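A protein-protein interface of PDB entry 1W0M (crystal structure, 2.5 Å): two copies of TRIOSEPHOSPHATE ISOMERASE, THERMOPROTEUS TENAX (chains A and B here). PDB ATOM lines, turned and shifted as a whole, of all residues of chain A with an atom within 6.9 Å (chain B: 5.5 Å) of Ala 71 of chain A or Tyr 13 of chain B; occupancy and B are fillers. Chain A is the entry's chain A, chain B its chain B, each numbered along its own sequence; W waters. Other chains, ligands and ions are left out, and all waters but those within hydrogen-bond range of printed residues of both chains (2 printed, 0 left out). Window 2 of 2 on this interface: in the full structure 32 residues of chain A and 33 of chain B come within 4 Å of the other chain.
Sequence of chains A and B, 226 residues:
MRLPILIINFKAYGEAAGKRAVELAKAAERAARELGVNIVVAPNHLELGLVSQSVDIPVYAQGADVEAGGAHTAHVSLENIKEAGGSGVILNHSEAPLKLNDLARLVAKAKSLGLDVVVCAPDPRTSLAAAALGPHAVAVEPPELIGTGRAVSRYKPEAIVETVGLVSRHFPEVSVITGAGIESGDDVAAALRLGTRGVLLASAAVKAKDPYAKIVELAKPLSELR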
ATOM      1  N   ALA A  68     -12.850  -3.524   5.826  1.00  0.00           N
ATOM      2  CA  ALA A  68     -13.043  -3.285   4.405  1.00  0.00           C
ATOM      3  C   ALA A  68     -12.122  -2.231   3.781  1.00  0.00           C
ATOM      4  O   ALA A  68     -11.480  -1.440   4.485  1.00  0.00           O
ATOM      5  CB  ALA A  68     -14.493  -2.922   4.159  1.00  0.00           C
ATOM      6  N   GLY A  69     -12.051  -2.235   2.451  1.00  0.00           N
ATOM      7  CA  GLY A  69     -11.215  -1.282   1.753  1.00  0.00           C
ATOM      8  C   GLY A  69     -11.730   0.128   2.015  1.00  0.00           C
ATOM      9  O   GLY A  69     -12.788   0.309   2.626  1.00  0.00           O
ATOM     10  N   GLY A  70     -10.983   1.130   1.565  1.00  0.00           N
ATOM     11  CA  GLY A  70     -11.399   2.497   1.782  1.00  0.00           C
ATOM     12  C   GLY A  70     -10.201   3.376   2.064  1.00  0.00           C
ATOM     13  O   GLY A  70      -9.055   2.997   1.780  1.00  0.00           O
ATOM     14  N   ALA A  71     -10.483   4.541   2.639  1.00  0.00           N
ATOM     15  CA  ALA A  71      -9.485   5.535   2.978  1.00  0.00           C
ATOM     16  C   ALA A  71      -8.766   5.194   4.289  1.00  0.00           C
ATOM     17  O   ALA A  71      -8.934   5.878   5.307  1.00  0.00           O
ATOM     18  CB  ALA A  71     -10.147   6.903   3.074  1.00  0.00           C
ATOM     19  N   HIS A  72      -7.957   4.141   4.250  1.00  0.00           N
ATOM     20  CA  HIS A  72      -7.198   3.697   5.417  1.00  0.00           C
ATOM     21  C   HIS A  72      -5.729   3.571   5.045  1.00  0.00           C
ATOM     22  O   HIS A  72      -5.175   2.475   5.005  1.00  0.00           O
ATOM     23  CB  HIS A  72      -7.721   2.353   5.909  1.00  0.00           C
ATOM     24  CG  HIS A  72      -9.203   2.322   6.086  1.00  0.00           C
ATOM     25  ND1 HIS A  72      -9.851   3.096   7.027  1.00  0.00           N
ATOM     26  CD2 HIS A  72     -10.170   1.649   5.410  1.00  0.00           C
ATOM     27  CE1 HIS A  72     -11.154   2.903   6.924  1.00  0.00           C
ATOM     28  NE2 HIS A  72     -11.374   2.031   5.950  1.00  0.00           N
ATOM     29  N   THR A  73      -5.114   4.710   4.763  1.00  0.00           N
ATOM     30  CA  THR A  73      -3.704   4.761   4.407  1.00  0.00           C
ATOM     31  C   THR A  73      -2.847   4.004   5.429  1.00  0.00           C
ATOM     32  O   THR A  73      -3.010   4.166   6.633  1.00  0.00           O
ATOM     33  CB  THR A  73      -3.204   6.230   4.356  1.00  0.00           C
ATOM     34  OG1 THR A  73      -3.976   6.974   3.400  1.00  0.00           O
ATOM     35  CG2 THR A  73      -1.739   6.284   3.969  1.00  0.00           C
ATOM     36  N   HIS A  75      -2.908   0.975   6.281  1.00  0.00           N
ATOM     37  CA  HIS A  75      -3.600  -0.089   7.005  1.00  0.00           C
ATOM     38  C   HIS A  75      -3.750  -1.317   6.129  1.00  0.00           C
ATOM     39  O   HIS A  75      -3.666  -1.240   4.916  1.00  0.00           O
ATOM     40  CB  HIS A  75      -4.980   0.394   7.448  1.00  0.00           C
ATOM     41  CG  HIS A  75      -4.924   1.473   8.481  1.00  0.00           C
ATOM     42  ND1 HIS A  75      -4.602   1.223   9.797  1.00  0.00           N
ATOM     43  CD2 HIS A  75      -5.039   2.814   8.369  1.00  0.00           C
ATOM     44  CE1 HIS A  75      -4.520   2.367  10.451  1.00  0.00           C
ATOM     45  NE2 HIS A  75      -4.779   3.348   9.607  1.00  0.00           N
ATOM     46  N   ASN A  80      -8.653  -6.258   1.259  1.00  0.00           N
ATOM     47  CA  ASN A  80      -7.449  -6.115   0.451  1.00  0.00           C
ATOM     48  C   ASN A  80      -6.612  -7.390   0.492  1.00  0.00           C
ATOM     49  O   ASN A  80      -5.929  -7.721  -0.476  1.00  0.00           O
ATOM     50  CB  ASN A  80      -6.597  -4.936   0.941  1.00  0.00           C
ATOM     51  CG  ASN A  80      -7.166  -3.576   0.530  1.00  0.00           C
ATOM     52  OD1 ASN A  80      -6.643  -2.556   0.935  1.00  0.00           O
ATOM     53  ND2 ASN A  80      -8.229  -3.565  -0.276  1.00  0.00           N
ATOM     54  N   GLU A  83      -8.163  -9.539  -1.961  1.00  0.00           N
ATOM     55  CA  GLU A  83      -7.899  -9.008  -3.286  1.00  0.00           C
ATOM     56  C   GLU A  83      -6.442  -9.245  -3.719  1.00  0.00           C
ATOM     57  O   GLU A  83      -6.152  -9.380  -4.917  1.00  0.00           O
ATOM     58  CB  GLU A  83      -8.274  -7.513  -3.335  1.00  0.00           C
ATOM     59  CG  GLU A  83      -9.803  -7.287  -3.205  1.00  0.00           C
ATOM     60  CD  GLU A  83     -10.236  -5.848  -2.790  1.00  0.00           C
ATOM     61  OE1 GLU A  83      -9.607  -5.237  -1.885  1.00  0.00           O
ATOM     62  OE2 GLU A  83     -11.239  -5.337  -3.363  1.00  0.00           O
ATOM     63  N   ASN B   9      -1.496   8.303  -3.744  1.00  0.00           N
ATOM     64  CA  ASN B   9      -1.679   7.431  -2.592  1.00  0.00           C
ATOM     65  C   ASN B   9      -2.880   6.519  -2.874  1.00  0.00           C
ATOM     66  O   ASN B   9      -4.006   6.993  -2.952  1.00  0.00           O
ATOM     67  CB  ASN B   9      -1.932   8.306  -1.370  1.00  0.00           C
ATOM     68  CG  ASN B   9      -2.222   7.510  -0.105  1.00  0.00           C
ATOM     69  OD1 ASN B   9      -2.133   6.286  -0.081  1.00  0.00           O
ATOM     70  ND2 ASN B   9      -2.566   8.226   0.965  1.00  0.00           N
ATOM     71  N   PHE B  10      -2.635   5.218  -3.050  1.00  0.00           N
ATOM     72  CA  PHE B  10      -3.699   4.259  -3.340  1.00  0.00           C
ATOM     73  C   PHE B  10      -4.570   3.950  -2.105  1.00  0.00           C
ATOM     74  O   PHE B  10      -5.646   3.340  -2.230  1.00  0.00           O
ATOM     75  CB  PHE B  10      -3.106   2.922  -3.826  1.00  0.00           C
ATOM     76  CG  PHE B  10      -2.388   2.985  -5.162  1.00  0.00           C
ATOM     77  CD1 PHE B  10      -2.111   4.204  -5.785  1.00  0.00           C
ATOM     78  CD2 PHE B  10      -1.959   1.799  -5.784  1.00  0.00           C
ATOM     79  CE1 PHE B  10      -1.416   4.247  -7.017  1.00  0.00           C
ATOM     80  CE2 PHE B  10      -1.266   1.825  -7.009  1.00  0.00           C
ATOM     81  CZ  PHE B  10      -0.991   3.057  -7.631  1.00  0.00           C
ATOM     82  N   LYS B  11      -4.089   4.355  -0.925  1.00  0.00           N
ATOM     83  CA  LYS B  11      -4.753   4.041   0.338  1.00  0.00           C
ATOM     84  C   LYS B  11      -5.125   2.545   0.321  1.00  0.00           C
ATOM     85  O   LYS B  11      -4.353   1.716  -0.192  1.00  0.00           O
ATOM     86  CB  LYS B  11      -5.980   4.935   0.536  1.00  0.00           C
ATOM     87  CG  LYS B  11      -5.613   6.413   0.539  1.00  0.00           C
ATOM     88  CD  LYS B  11      -6.710   7.300   1.099  1.00  0.00           C
ATOM     89  CE  LYS B  11      -6.187   8.717   1.245  1.00  0.00           C
ATOM     90  NZ  LYS B  11      -7.180   9.653   1.811  1.00  0.00           N
ATOM     91  N   ALA B  12      -6.282   2.191   0.875  1.00  0.00           N
ATOM     92  CA  ALA B  12      -6.716   0.790   0.892  1.00  0.00           C
ATOM     93  C   ALA B  12      -7.894   0.570  -0.057  1.00  0.00           C
ATOM     94  O   ALA B  12      -8.638  -0.394   0.090  1.00  0.00           O
ATOM     95  CB  ALA B  12      -7.122   0.385   2.303  1.00  0.00           C
ATOM     96  N   TYR B  13      -8.073   1.469  -1.015  1.00  0.00           N
ATOM     97  CA  TYR B  13      -9.169   1.361  -1.973  1.00  0.00           C
ATOM     98  C   TYR B  13      -9.146   0.064  -2.764  1.00  0.00           C
ATOM     99  O   TYR B  13      -8.095  -0.350  -3.277  1.00  0.00           O
ATOM    100  CB  TYR B  13      -9.110   2.525  -2.958  1.00  0.00           C
ATOM    101  CG  TYR B  13      -9.471   3.852  -2.367  1.00  0.00           C
ATOM    102  CD1 TYR B  13      -8.584   4.926  -2.418  1.00  0.00           C
ATOM    103  CD2 TYR B  13     -10.721   4.057  -1.800  1.00  0.00           C
ATOM    104  CE1 TYR B  13      -8.942   6.193  -1.907  1.00  0.00           C
ATOM    105  CE2 TYR B  13     -11.085   5.311  -1.291  1.00  0.00           C
ATOM    106  CZ  TYR B  13     -10.196   6.369  -1.343  1.00  0.00           C
ATOM    107  OH  TYR B  13     -10.559   7.587  -0.793  1.00  0.00           O
ATOM    108  N   GLY B  14     -10.300  -0.586  -2.863  1.00  0.00           N
ATOM    109  CA  GLY B  14     -10.379  -1.808  -3.653  1.00  0.00           C
ATOM    110  C   GLY B  14     -10.111  -1.513  -5.135  1.00  0.00           C
ATOM    111  O   GLY B  14      -9.587  -2.354  -5.857  1.00  0.00           O
ATOM    112  N   GLU B  15     -10.457  -0.312  -5.600  1.00  0.00           N
ATOM    113  CA  GLU B  15     -10.226   0.056  -6.999  1.00  0.00           C
ATOM    114  C   GLU B  15      -8.732   0.007  -7.336  1.00  0.00           C
ATOM    115  O   GLU B  15      -8.358  -0.023  -8.517  1.00  0.00           O
ATOM    116  CB  GLU B  15     -10.752   1.477  -7.296  1.00  0.00           C
ATOM    117  CG  GLU B  15     -12.249   1.676  -7.078  1.00  0.00           C
ATOM    118  CD  GLU B  15     -12.609   2.073  -5.633  1.00  0.00           C
ATOM    119  OE1 GLU B  15     -12.064   1.475  -4.661  1.00  0.00           O
ATOM    120  OE2 GLU B  15     -13.454   2.983  -5.464  1.00  0.00           O
ATOM    121  N   ALA B  16      -7.879   0.014  -6.307  1.00  0.00           N
ATOM    122  CA  ALA B  16      -6.441  -0.026  -6.532  1.00  0.00           C
ATOM    123  C   ALA B  16      -5.770  -1.244  -5.913  1.00  0.00           C
ATOM    124  O   ALA B  16      -4.546  -1.295  -5.825  1.00  0.00           O
ATOM    125  CB  ALA B  16      -5.801   1.227  -5.999  1.00  0.00           C
ATOM    126  N   ALA B  17      -6.564  -2.233  -5.508  1.00  0.00           N
ATOM    127  CA  ALA B  17      -6.016  -3.421  -4.857  1.00  0.00           C
ATOM    128  C   ALA B  17      -5.740  -4.557  -5.834  1.00  0.00           C
ATOM    129  O   ALA B  17      -6.181  -4.516  -6.988  1.00  0.00           O
ATOM    130  CB  ALA B  17      -6.962  -3.885  -3.769  1.00  0.00           C
ATOM    131  N   ASN B  44      -1.084  -0.047  -1.473  1.00  0.00           N
ATOM    132  CA  ASN B  44      -1.265  -0.540  -0.119  1.00  0.00           C
ATOM    133  C   ASN B  44      -0.101  -1.518   0.161  1.00  0.00           C
ATOM    134  O   ASN B  44       0.516  -2.071  -0.758  1.00  0.00           O
ATOM    135  CB  ASN B  44      -2.650  -1.193   0.087  1.00  0.00           C
ATOM    136  CG  ASN B  44      -2.785  -2.566  -0.562  1.00  0.00           C
ATOM    137  OD1 ASN B  44      -1.891  -3.403  -0.465  1.00  0.00           O
ATOM    138  ND2 ASN B  44      -3.940  -2.819  -1.192  1.00  0.00           N
ATOM    139  N   GLU B  95      -4.715   9.245   8.381  1.00  0.00           N
ATOM    140  CA  GLU B  95      -5.348   7.959   8.581  1.00  0.00           C
ATOM    141  C   GLU B  95      -4.494   6.972   9.364  1.00  0.00           C
ATOM    142  O   GLU B  95      -4.992   5.930   9.806  1.00  0.00           O
ATOM    143  CB  GLU B  95      -5.737   7.385   7.208  1.00  0.00           C
ATOM    144  CG  GLU B  95      -6.883   8.175   6.571  1.00  0.00           C
ATOM    145  CD  GLU B  95      -6.882   8.163   5.051  1.00  0.00           C
ATOM    146  OE1 GLU B  95      -6.268   7.258   4.444  1.00  0.00           O
ATOM    147  OE2 GLU B  95      -7.526   9.063   4.464  1.00  0.00           O
ATOM    148  N   GLY B 147     -10.639  13.545   0.649  1.00  0.00           N
ATOM    149  CA  GLY B 147     -11.668  12.795  -0.050  1.00  0.00           C
ATOM    150  C   GLY B 147     -12.919  13.576  -0.406  1.00  0.00           C
ATOM    151  O   GLY B 147     -13.874  12.999  -0.909  1.00  0.00           O
ATOM    152  N   ALA B 202      -5.307  11.173  -3.818  1.00  0.00           N
ATOM    153  CA  ALA B 202      -5.750   9.797  -3.883  1.00  0.00           C
ATOM    154  C   ALA B 202      -7.017   9.595  -4.725  1.00  0.00           C
ATOM    155  O   ALA B 202      -6.953   9.016  -5.805  1.00  0.00           O
ATOM    156  CB  ALA B 202      -5.961   9.261  -2.450  1.00  0.00           C
ATOM    157  N   SER B 203      -8.151  10.065  -4.216  1.00  0.00           N
ATOM    158  CA  SER B 203      -9.458   9.925  -4.870  1.00  0.00           C
ATOM    159  C   SER B 203      -9.486  10.160  -6.377  1.00  0.00           C
ATOM    160  O   SER B 203      -9.804   9.259  -7.156  1.00  0.00           O
ATOM    161  CB  SER B 203     -10.473  10.888  -4.237  1.00  0.00           C
ATOM    162  OG  SER B 203     -10.764  10.536  -2.911  1.00  0.00           O
ATOM    163  N   VAL B 206      -7.370   7.461  -8.158  1.00  0.00           N
ATOM    164  CA  VAL B 206      -7.821   6.109  -7.882  1.00  0.00           C
ATOM    165  C   VAL B 206      -9.225   5.798  -8.384  1.00  0.00           C
ATOM    166  O   VAL B 206      -9.513   4.687  -8.833  1.00  0.00           O
ATOM    167  CB  VAL B 206      -7.720   5.804  -6.352  1.00  0.00           C
ATOM    168  CG1 VAL B 206      -8.372   4.454  -6.020  1.00  0.00           C
ATOM    169  CG2 VAL B 206      -6.248   5.787  -5.935  1.00  0.00           C
ATOM    170  N   LYS B 207     -10.100   6.786  -8.332  1.00  0.00           N
ATOM    171  CA  LYS B 207     -11.460   6.541  -8.749  1.00  0.00           C
ATOM    172  C   LYS B 207     -11.832   7.039 -10.137  1.00  0.00           C
ATOM    173  O   LYS B 207     -12.992   6.959 -10.530  1.00  0.00           O
ATOM    174  CB  LYS B 207     -12.401   7.087  -7.675  1.00  0.00           C
ATOM    175  CG  LYS B 207     -12.340   6.235  -6.423  1.00  0.00           C
ATOM    176  CD  LYS B 207     -13.238   6.694  -5.310  1.00  0.00           C
ATOM    177  CE  LYS B 207     -13.211   5.649  -4.225  1.00  0.00           C
ATOM    178  NZ  LYS B 207     -14.091   5.970  -3.095  1.00  0.00           N
HETATM  179  O   HOH W   1      -4.368   4.266  12.696  1.00  0.00           O
HETATM  180  O   HOH W   2      -4.736  -5.417  -2.011  1.00  0.00           O
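N of Ala 12 of chain B sits at hydrogen-bond distance from O of Gly 70 of chain A (3.0 Å).
N of Tyr 13 of chain B lies within hydrogen-bond range of O of Gly 70 of chain A.
The side-chain amide nitrogen (ND2) of Asn 9 of chain B is in hydrogen-bond range of the side-chain hydroxyl (OG1) of Thr 73 of chain A, 3.1 Å away.
OG1 of Thr 73 of chain A lies within hydrogen-bond range of OE1 of Glu 95 of chain B.
The backbone carbonyl oxygen (O) of Glu 95 of chain B sits at hydrogen-bond distance from a ring nitrogen (NE2) of His 75 of chain A (2.6 Å).
OD1 of Asn 80 of chain A lies close to O of Ala 12 of chain B, 3.1 Å away.
The side-chain amide oxygen (OD1) of Asn 80 of chain A is in hydrogen-bond range of the side-chain amide nitrogen (ND2) of Asn 44 of chain B, 3.4 Å away.
The side-chain carboxylate (OE1) of Glu 95 of chain B sits close to the backbone carbonyl oxygen (O) of Ala 71 of chain A, at 3.1 Å.
Of the 9 printed residues of chain A, 8 touch a printed residue of chain B.
Hydrophobic or aromatic side chains of chain A within 4 Å of the printed part of chain B: Ala 71 and His 75.
Of the 16 printed residues of chain B, 8 touch a printed residue of chain A.
Hydrophobic or aromatic side chains of chain B within 4 Å of the printed part of chain A: Ala 12, Tyr 13 and Ala 17.
Along chain B the printed residues that touch a printed residue of chain A span positions 9 to 95.
ND2 of Asn 80 of chain A lies within hydrogen-bond range of OE1 of Glu 83 of chain A, at 2.7 Å.
The side-chain amide oxygen (OD1) of Asn 9 of chain B lies within hydrogen-bond range of the backbone NH (N) of Lys 11 of chain B, 2.9 Å away.
The side-chain carboxylate (OE2) of Glu 95 of chain B lies within salt-bridge range of the side-chain amino group (NZ) of Lys 11 of chain B, at 2.7 Å.
Water W2 lies within hydrogen-bond range of the side-chain amide nitrogen (ND2) of Asn 44 of chain B (2.8 Å) and the backbone carbonyl oxygen (O) of Asn 80 of chain A (3.0 Å).
Water W1 bridges NE2 of His 75 of chain A (3.2 Å) and O of Glu 95 of chain B (3.4 Å).
Gly 69 of chain A touches Ala 12 of chain B (CA to O, 3.2 Å).
O of Gly 70 of chain A touches CB of Lys 11 of chain B, 3.8 Å away.
Lys 11 of chain B touches Ala 71 of chain A.
Ala 71 of chain A touches Tyr 13 of chain B.
O of His 72 of chain A touches CB of Ala 12 of chain B (3.9 Å).
N of His 72 of chain A touches OE1 of Glu 95 of chain B, at 3.6 Å.
Thr 73 of chain A touches Lys 11 of chain B.
Asn 80 of chain A touches Ala 17 of chain B (ND2 to CB, 3.7 Å).
Glu 83 of chain A touches Gly 14 of chain B (OE2 to CA, 3.6 Å).
Glu 83 of chain A touches Ala 17 of chain B.
No position is printed for both chains.
Ala 71 of chain A touches just these residues of chain B: Lys 11 (3.8 Å), Tyr 13 (3.9 Å) and Glu 95 (3.1 Å).
Of the printed residues of chain B, Thr 73 of chain A touches Asn 9, Lys 11 and Glu 95.
Of the printed residues of chain A, Asn 9 of chain B touches Thr 73 (3.1 Å).
Phe 10 of chain B touches none of the printed residues of chain A.
Ala 16 of chain B touches none of the printed residues of chain A.
Of the printed residues of chain A, Asn 44 of chain B touches Asn 80.
Of the printed residues of chain A, Glu 95 of chain B touches Ala 71 (3.1 Å), His 72 (3.6 Å), Thr 73 (2.5 Å) and His 75 (2.6 Å).
The nearest residue of chain B that does not touch Ala 71 of chain A is Ala 12 of chain B (5.1 Å).
The nearest printed residue of chain B that does not touch His 72 of chain A is Lys 11 of chain B (4.3 Å).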
